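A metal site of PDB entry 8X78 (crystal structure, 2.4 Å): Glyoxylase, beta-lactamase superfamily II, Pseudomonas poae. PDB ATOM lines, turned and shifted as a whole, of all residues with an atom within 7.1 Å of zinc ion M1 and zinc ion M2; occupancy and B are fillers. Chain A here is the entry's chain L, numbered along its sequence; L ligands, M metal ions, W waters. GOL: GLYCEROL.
A ring nitrogen (NE2) of His 109 lies within hydrogen-bond range of the side-chain amide oxygen (OE1) of Gln 235, at 2.9 Å.
ND1 of His 112 lies within hydrogen-bond range of OD2 of Asp 66 (2.6 Å).
The backbone NH (N) of His 263 sits at hydrogen-bond distance from the backbone carbonyl oxygen (O) of Tyr 220 (3.1 Å).
The side-chain sulfur of Met 46 sits close to a ring nitrogen (ND1) of His 263, at 3.6 Å.
A ring nitrogen (NE2) of His 107 lies close to the side-chain carboxylate of Asp 217 (2.6 Å).
The backbone carbonyl oxygen (O) of His 196 lies within hydrogen-bond range of the backbone NH (N) of Gln 235 (3.0 Å).
The backbone carbonyl oxygen of Asp 111 is in hydrogen-bond range of the side-chain hydroxyl of Tyr 20, 3.1 Å away.
A ring nitrogen (ND1) of His 107 sits at hydrogen-bond distance from the side-chain hydroxyl of Thr 106, 3.0 Å away.
Tyr 220 touches zinc ion M1.
Within 4 Å of zinc ion M1: His 107, His 109, His 196, Asp 217 and Tyr 220.
The nearest printed residue that does not touch zinc ion M1 is His 112 (4.7 Å).
Of the 24 residues printed, 4 come within 4 Å of zinc ion M2.
ND1 of His 109 is bound to zinc ion M1 (1.9 Å).
Zinc ion M1 is bound by OD2 of Asp 217 (2.3 Å).
NE2 of His 196 binds zinc ion M1, 2.3 Å away.
Slightly farther from zinc ion M1 lies a ring nitrogen (NE2) of His 107 (2.6 Å).
Zinc ion M2 is bound by water W1, 1.9 Å away.
A ring nitrogen (NE2) of His 112 binds zinc ion M2 (2.2 Å).
NE2 of His 263 is bound to zinc ion M2 (2.3 Å).
Zinc ion M2 is bound by OD2 of Asp 217, 2.3 Å away.
OD2 of Asp 111 is bound to zinc ion M2 (2.6 Å).
Slightly farther from zinc ion M2 lies O2 of the ligand (2.8 Å).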
ATOM      1  N   TYR A  20      -4.936  30.566 -11.394  1.00  0.00           N
ATOM      2  CA  TYR A  20      -5.552  31.848 -11.737  1.00  0.00           C
ATOM      3  C   TYR A  20      -4.887  33.017 -11.053  1.00  0.00           C
ATOM      4  O   TYR A  20      -5.231  34.173 -11.364  1.00  0.00           O
ATOM      5  CB  TYR A  20      -7.052  31.842 -11.380  1.00  0.00           C
ATOM      6  CG  TYR A  20      -7.332  31.804  -9.893  1.00  0.00           C
ATOM      7  CD1 TYR A  20      -7.353  30.588  -9.190  1.00  0.00           C
ATOM      8  CD2 TYR A  20      -7.584  32.981  -9.174  1.00  0.00           C
ATOM      9  CE1 TYR A  20      -7.620  30.554  -7.821  1.00  0.00           C
ATOM     10  CE2 TYR A  20      -7.857  32.944  -7.813  1.00  0.00           C
ATOM     11  CZ  TYR A  20      -7.865  31.731  -7.143  1.00  0.00           C
ATOM     12  OH  TYR A  20      -8.127  31.699  -5.790  1.00  0.00           O
ATOM     13  N   PHE A  30       2.071  27.325   4.855  1.00  0.00           N
ATOM     14  CA  PHE A  30       1.537  26.179   4.147  1.00  0.00           C
ATOM     15  C   PHE A  30       2.175  24.860   4.587  1.00  0.00           C
ATOM     16  O   PHE A  30       1.528  23.816   4.515  1.00  0.00           O
ATOM     17  CB  PHE A  30       1.754  26.350   2.638  1.00  0.00           C
ATOM     18  CG  PHE A  30       0.964  27.487   2.012  1.00  0.00           C
ATOM     19  CD1 PHE A  30      -0.421  27.544   2.146  1.00  0.00           C
ATOM     20  CD2 PHE A  30       1.607  28.456   1.241  1.00  0.00           C
ATOM     21  CE1 PHE A  30      -1.148  28.564   1.550  1.00  0.00           C
ATOM     22  CE2 PHE A  30       0.889  29.496   0.644  1.00  0.00           C
ATOM     23  CZ  PHE A  30      -0.488  29.550   0.799  1.00  0.00           C
ATOM     24  N   MET A  46      -2.518  29.877  -6.740  1.00  0.00           N
ATOM     25  CA  MET A  46      -3.939  29.868  -6.416  1.00  0.00           C
ATOM     26  C   MET A  46      -4.619  29.106  -7.552  1.00  0.00           C
ATOM     27  O   MET A  46      -4.426  29.433  -8.727  1.00  0.00           O
ATOM     28  CB  MET A  46      -4.481  31.295  -6.260  1.00  0.00           C
ATOM     29  CG  MET A  46      -3.578  32.162  -5.364  1.00  0.00           C
ATOM     30  SD  MET A  46      -3.643  31.721  -3.604  1.00  0.00           S
ATOM     31  CE  MET A  46      -5.402  31.961  -3.330  1.00  0.00           C
ATOM     32  N   ASP A  66     -13.830  24.273  -6.693  1.00  0.00           N
ATOM     33  CA  ASP A  66     -13.460  25.623  -6.303  1.00  0.00           C
ATOM     34  C   ASP A  66     -13.414  26.529  -7.528  1.00  0.00           C
ATOM     35  O   ASP A  66     -13.399  26.070  -8.681  1.00  0.00           O
ATOM     36  CB  ASP A  66     -12.134  25.597  -5.553  1.00  0.00           C
ATOM     37  CG  ASP A  66     -12.220  24.822  -4.230  1.00  0.00           C
ATOM     38  OD1 ASP A  66     -13.345  24.697  -3.686  1.00  0.00           O
ATOM     39  OD2 ASP A  66     -11.182  24.289  -3.761  1.00  0.00           O
ATOM     40  N   THR A 106     -14.679  22.925  -1.823  1.00  0.00           N
ATOM     41  CA  THR A 106     -13.953  22.232  -0.749  1.00  0.00           C
ATOM     42  C   THR A 106     -14.235  22.875   0.603  1.00  0.00           C
ATOM     43  O   THR A 106     -14.437  22.168   1.593  1.00  0.00           O
ATOM     44  CB  THR A 106     -12.447  22.222  -1.044  1.00  0.00           C
ATOM     45  OG1 THR A 106     -11.972  23.553  -1.265  1.00  0.00           O
ATOM     46  CG2 THR A 106     -12.121  21.375  -2.252  1.00  0.00           C
ATOM     47  N   HIS A 107     -14.281  24.212   0.660  1.00  0.00           N
ATOM     48  CA  HIS A 107     -14.514  24.957   1.898  1.00  0.00           C
ATOM     49  C   HIS A 107     -14.789  26.411   1.550  1.00  0.00           C
ATOM     50  O   HIS A 107     -14.587  26.848   0.414  1.00  0.00           O
ATOM     51  CB  HIS A 107     -13.335  24.815   2.885  1.00  0.00           C
ATOM     52  CG  HIS A 107     -12.044  25.427   2.408  1.00  0.00           C
ATOM     53  ND1 HIS A 107     -11.443  25.085   1.223  1.00  0.00           N
ATOM     54  CD2 HIS A 107     -11.198  26.293   3.023  1.00  0.00           C
ATOM     55  CE1 HIS A 107     -10.284  25.731   1.102  1.00  0.00           C
ATOM     56  NE2 HIS A 107     -10.121  26.474   2.183  1.00  0.00           N
ATOM     57  N   MET A 108     -15.274  27.172   2.530  1.00  0.00           N
ATOM     58  CA  MET A 108     -15.789  28.509   2.255  1.00  0.00           C
ATOM     59  C   MET A 108     -14.753  29.617   2.476  1.00  0.00           C
ATOM     60  O   MET A 108     -15.135  30.796   2.592  1.00  0.00           O
ATOM     61  CB  MET A 108     -17.048  28.766   3.092  1.00  0.00           C
ATOM     62  CG  MET A 108     -18.276  28.041   2.505  1.00  0.00           C
ATOM     63  SD  MET A 108     -19.773  28.163   3.494  1.00  0.00           S
ATOM     64  CE  MET A 108     -20.131  29.926   3.276  1.00  0.00           C
ATOM     65  N   HIS A 109     -13.464  29.289   2.483  1.00  0.00           N
ATOM     66  CA  HIS A 109     -12.471  30.355   2.419  1.00  0.00           C
ATOM     67  C   HIS A 109     -12.661  31.142   1.132  1.00  0.00           C
ATOM     68  O   HIS A 109     -13.051  30.599   0.099  1.00  0.00           O
ATOM     69  CB  HIS A 109     -11.069  29.763   2.490  1.00  0.00           C
ATOM     70  CG  HIS A 109     -10.626  29.415   3.884  1.00  0.00           C
ATOM     71  ND1 HIS A 109      -9.492  28.668   4.144  1.00  0.00           N
ATOM     72  CD2 HIS A 109     -11.171  29.707   5.092  1.00  0.00           C
ATOM     73  CE1 HIS A 109      -9.346  28.539   5.451  1.00  0.00           C
ATOM     74  NE2 HIS A 109     -10.360  29.148   6.043  1.00  0.00           N
ATOM     75  N   PHE A 110     -12.365  32.447   1.194  1.00  0.00           N
ATOM     76  CA  PHE A 110     -12.690  33.373   0.106  1.00  0.00           C
ATOM     77  C   PHE A 110     -12.110  32.907  -1.217  1.00  0.00           C
ATOM     78  O   PHE A 110     -12.725  33.080  -2.278  1.00  0.00           O
ATOM     79  CB  PHE A 110     -12.186  34.767   0.427  1.00  0.00           C
ATOM     80  CG  PHE A 110     -10.697  34.904   0.320  1.00  0.00           C
ATOM     81  CD1 PHE A 110      -9.873  34.410   1.314  1.00  0.00           C
ATOM     82  CD2 PHE A 110     -10.123  35.540  -0.776  1.00  0.00           C
ATOM     83  CE1 PHE A 110      -8.505  34.530   1.223  1.00  0.00           C
ATOM     84  CE2 PHE A 110      -8.752  35.668  -0.872  1.00  0.00           C
ATOM     85  CZ  PHE A 110      -7.940  35.169   0.130  1.00  0.00           C
ATOM     86  N   ASP A 111     -10.907  32.357  -1.190  1.00  0.00           N
ATOM     87  CA  ASP A 111     -10.239  31.997  -2.421  1.00  0.00           C
ATOM     88  C   ASP A 111     -10.712  30.654  -2.984  1.00  0.00           C
ATOM     89  O   ASP A 111     -10.116  30.168  -3.958  1.00  0.00           O
ATOM     90  CB  ASP A 111      -8.728  31.957  -2.210  1.00  0.00           C
ATOM     91  CG  ASP A 111      -8.318  30.976  -1.140  1.00  0.00           C
ATOM     92  OD1 ASP A 111      -8.952  30.941  -0.054  1.00  0.00           O
ATOM     93  OD2 ASP A 111      -7.318  30.261  -1.383  1.00  0.00           O
ATOM     94  N   HIS A 112     -11.744  30.018  -2.396  1.00  0.00           N
ATOM     95  CA  HIS A 112     -12.314  28.838  -3.009  1.00  0.00           C
ATOM     96  C   HIS A 112     -13.776  28.983  -3.396  1.00  0.00           C
ATOM     97  O   HIS A 112     -14.216  28.275  -4.303  1.00  0.00           O
ATOM     98  CB  HIS A 112     -12.112  27.644  -2.081  1.00  0.00           C
ATOM     99  CG  HIS A 112     -10.669  27.334  -1.867  1.00  0.00           C
ATOM    100  ND1 HIS A 112     -10.018  26.366  -2.603  1.00  0.00           N
ATOM    101  CD2 HIS A 112      -9.725  27.936  -1.107  1.00  0.00           C
ATOM    102  CE1 HIS A 112      -8.736  26.357  -2.270  1.00  0.00           C
ATOM    103  NE2 HIS A 112      -8.541  27.293  -1.361  1.00  0.00           N
ATOM    104  N   SER A 156      -9.119  34.411   6.268  1.00  0.00           N
ATOM    105  CA  SER A 156      -9.425  33.757   4.995  1.00  0.00           C
ATOM    106  C   SER A 156     -10.905  33.697   4.718  1.00  0.00           C
ATOM    107  O   SER A 156     -11.320  32.963   3.817  1.00  0.00           O
ATOM    108  CB  SER A 156      -8.864  32.326   4.975  1.00  0.00           C
ATOM    109  OG  SER A 156      -7.447  32.314   5.013  1.00  0.00           O
ATOM    110  N   HIS A 196      -9.400  21.095   7.825  1.00  0.00           N
ATOM    111  CA  HIS A 196      -8.975  22.466   7.522  1.00  0.00           C
ATOM    112  C   HIS A 196      -9.968  23.498   8.047  1.00  0.00           C
ATOM    113  O   HIS A 196      -9.567  24.556   8.536  1.00  0.00           O
ATOM    114  CB  HIS A 196      -8.774  22.670   6.022  1.00  0.00           C
ATOM    115  CG  HIS A 196      -8.245  24.026   5.675  1.00  0.00           C
ATOM    116  ND1 HIS A 196      -6.977  24.429   6.014  1.00  0.00           N
ATOM    117  CD2 HIS A 196      -8.840  25.078   5.075  1.00  0.00           C
ATOM    118  CE1 HIS A 196      -6.791  25.676   5.592  1.00  0.00           C
ATOM    119  NE2 HIS A 196      -7.908  26.084   5.019  1.00  0.00           N
ATOM    120  N   THR A 197     -11.268  23.206   7.929  1.00  0.00           N
ATOM    121  CA  THR A 197     -12.326  24.070   8.407  1.00  0.00           C
ATOM    122  C   THR A 197     -13.449  23.177   8.898  1.00  0.00           C
ATOM    123  O   THR A 197     -13.430  21.971   8.653  1.00  0.00           O
ATOM    124  CB  THR A 197     -12.864  25.025   7.312  1.00  0.00           C
ATOM    125  OG1 THR A 197     -13.367  24.257   6.208  1.00  0.00           O
ATOM    126  CG2 THR A 197     -11.783  26.021   6.796  1.00  0.00           C
ATOM    127  N   SER A 200     -14.787  21.086   5.847  1.00  0.00           N
ATOM    128  CA  SER A 200     -13.987  20.784   4.664  1.00  0.00           C
ATOM    129  C   SER A 200     -14.416  19.459   4.044  1.00  0.00           C
ATOM    130  O   SER A 200     -14.749  18.501   4.751  1.00  0.00           O
ATOM    131  CB  SER A 200     -12.504  20.727   5.030  1.00  0.00           C
ATOM    132  OG  SER A 200     -11.942  22.015   5.040  1.00  0.00           O
ATOM    133  N   GLY A 216      -8.326  20.120  -1.691  1.00  0.00           N
ATOM    134  CA  GLY A 216      -8.586  21.410  -1.092  1.00  0.00           C
ATOM    135  C   GLY A 216      -7.427  21.831  -0.235  1.00  0.00           C
ATOM    136  O   GLY A 216      -6.288  21.494  -0.525  1.00  0.00           O
ATOM    137  N   ASP A 217      -7.702  22.551   0.843  1.00  0.00           N
ATOM    138  CA  ASP A 217      -6.641  23.028   1.714  1.00  0.00           C
ATOM    139  C   ASP A 217      -6.283  22.072   2.805  1.00  0.00           C
ATOM    140  O   ASP A 217      -5.388  22.352   3.588  1.00  0.00           O
ATOM    141  CB  ASP A 217      -7.014  24.380   2.283  1.00  0.00           C
ATOM    142  CG  ASP A 217      -6.911  25.453   1.256  1.00  0.00           C
ATOM    143  OD1 ASP A 217      -6.151  25.290   0.276  1.00  0.00           O
ATOM    144  OD2 ASP A 217      -7.599  26.455   1.408  1.00  0.00           O
ATOM    145  N   ILE A 218      -7.007  20.968   2.933  1.00  0.00           N
ATOM    146  CA  ILE A 218      -6.571  19.926   3.852  1.00  0.00           C
ATOM    147  C   ILE A 218      -5.119  19.577   3.590  1.00  0.00           C
ATOM    148  O   ILE A 218      -4.319  19.412   4.515  1.00  0.00           O
ATOM    149  CB  ILE A 218      -7.457  18.676   3.727  1.00  0.00           C
ATOM    150  CG1 ILE A 218      -8.916  19.025   4.030  1.00  0.00           C
ATOM    151  CG2 ILE A 218      -6.945  17.580   4.693  1.00  0.00           C
ATOM    152  CD1 ILE A 218      -9.847  17.902   3.679  1.00  0.00           C
ATOM    153  N   TYR A 220      -2.338  21.523   1.849  1.00  0.00           N
ATOM    154  CA  TYR A 220      -1.778  22.696   1.186  1.00  0.00           C
ATOM    155  C   TYR A 220      -0.689  22.306   0.205  1.00  0.00           C
ATOM    156  O   TYR A 220      -0.674  22.745  -0.956  1.00  0.00           O
ATOM    157  CB  TYR A 220      -1.202  23.676   2.220  1.00  0.00           C
ATOM    158  CG  TYR A 220      -2.143  24.691   2.830  1.00  0.00           C
ATOM    159  CD1 TYR A 220      -3.196  25.237   2.110  1.00  0.00           C
ATOM    160  CD2 TYR A 220      -1.948  25.121   4.125  1.00  0.00           C
ATOM    161  CE1 TYR A 220      -4.038  26.180   2.675  1.00  0.00           C
ATOM    162  CE2 TYR A 220      -2.789  26.049   4.708  1.00  0.00           C
ATOM    163  CZ  TYR A 220      -3.825  26.587   3.981  1.00  0.00           C
ATOM    164  OH  TYR A 220      -4.641  27.529   4.580  1.00  0.00           O
ATOM    165  N   TYR A 233      -0.801  27.326   9.478  1.00  0.00           N
ATOM    166  CA  TYR A 233      -2.081  28.005   9.461  1.00  0.00           C
ATOM    167  C   TYR A 233      -3.153  27.019   9.010  1.00  0.00           C
ATOM    168  O   TYR A 233      -3.033  26.420   7.931  1.00  0.00           O
ATOM    169  CB  TYR A 233      -2.070  29.213   8.512  1.00  0.00           C
ATOM    170  CG  TYR A 233      -3.439  29.819   8.306  1.00  0.00           C
ATOM    171  CD1 TYR A 233      -3.955  30.725   9.216  1.00  0.00           C
ATOM    172  CD2 TYR A 233      -4.221  29.452   7.210  1.00  0.00           C
ATOM    173  CE1 TYR A 233      -5.216  31.282   9.038  1.00  0.00           C
ATOM    174  CE2 TYR A 233      -5.507  30.020   7.018  1.00  0.00           C
ATOM    175  CZ  TYR A 233      -5.978  30.925   7.950  1.00  0.00           C
ATOM    176  OH  TYR A 233      -7.220  31.494   7.805  1.00  0.00           O
ATOM    177  N   HIS A 234      -4.174  26.840   9.841  1.00  0.00           N
ATOM    178  CA  HIS A 234      -5.381  26.117   9.472  1.00  0.00           C
ATOM    179  C   HIS A 234      -6.436  26.488  10.500  1.00  0.00           C
ATOM    180  O   HIS A 234      -6.121  27.066  11.540  1.00  0.00           O
ATOM    181  CB  HIS A 234      -5.158  24.614   9.407  1.00  0.00           C
ATOM    182  CG  HIS A 234      -4.840  24.011  10.735  1.00  0.00           C
ATOM    183  ND1 HIS A 234      -5.791  23.789  11.698  1.00  0.00           N
ATOM    184  CD2 HIS A 234      -3.669  23.562  11.255  1.00  0.00           C
ATOM    185  CE1 HIS A 234      -5.231  23.251  12.764  1.00  0.00           C
ATOM    186  NE2 HIS A 234      -3.935  23.104  12.520  1.00  0.00           N
ATOM    187  N   GLN A 235      -7.698  26.178  10.209  1.00  0.00           N
ATOM    188  CA  GLN A 235      -8.756  26.587  11.129  1.00  0.00           C
ATOM    189  C   GLN A 235      -9.615  25.403  11.595  1.00  0.00           C
ATOM    190  O   GLN A 235     -10.800  25.544  11.885  1.00  0.00           O
ATOM    191  CB  GLN A 235      -9.592  27.701  10.503  1.00  0.00           C
ATOM    192  CG  GLN A 235      -8.720  28.896  10.110  1.00  0.00           C
ATOM    193  CD  GLN A 235      -9.535  30.139   9.789  1.00  0.00           C
ATOM    194  OE1 GLN A 235     -10.234  30.165   8.781  1.00  0.00           O
ATOM    195  NE2 GLN A 235      -9.468  31.142  10.651  1.00  0.00           N
ATOM    196  N   GLY A 262      -3.744  22.182  -2.585  1.00  0.00           N
ATOM    197  CA  GLY A 262      -4.355  23.487  -2.769  1.00  0.00           C
ATOM    198  C   GLY A 262      -3.477  24.596  -3.304  1.00  0.00           C
ATOM    199  O   GLY A 262      -3.933  25.424  -4.110  1.00  0.00           O
ATOM    200  N   HIS A 263      -2.217  24.641  -2.856  1.00  0.00           N
ATOM    201  CA  HIS A 263      -1.368  25.820  -2.999  1.00  0.00           C
ATOM    202  C   HIS A 263       0.104  25.437  -3.115  1.00  0.00           C
ATOM    203  O   HIS A 263       0.965  26.044  -2.478  1.00  0.00           O
ATOM    204  CB  HIS A 263      -1.535  26.722  -1.782  1.00  0.00           C
ATOM    205  CG  HIS A 263      -2.888  27.335  -1.672  1.00  0.00           C
ATOM    206  ND1 HIS A 263      -3.336  28.321  -2.528  1.00  0.00           N
ATOM    207  CD2 HIS A 263      -3.934  27.024  -0.865  1.00  0.00           C
ATOM    208  CE1 HIS A 263      -4.572  28.645  -2.201  1.00  0.00           C
ATOM    209  NE2 HIS A 263      -4.970  27.851  -1.211  1.00  0.00           N
HETATM  210  C1  GOL L   1      -5.488  31.624   2.418  1.00  0.00           C
HETATM  211  O1  GOL L   1      -4.815  32.656   3.110  1.00  0.00           O
HETATM  212  C2  GOL L   1      -4.459  30.754   1.620  1.00  0.00           C
HETATM  213  O2  GOL L   1      -4.996  29.463   1.415  1.00  0.00           O
HETATM  214  C3  GOL L   1      -4.157  31.549   0.310  1.00  0.00           C
HETATM  215  O3  GOL L   1      -3.396  32.677   0.673  1.00  0.00           O
HETATM  216 ZN    ZN M   1      -8.048  27.644   3.329  1.00  0.00          ZN
HETATM  217 ZN    ZN M   2      -6.921  28.080  -0.069  1.00  0.00          ZN
HETATM  218  O   HOH W   1      -7.503  29.481   1.139  1.00  0.00           O
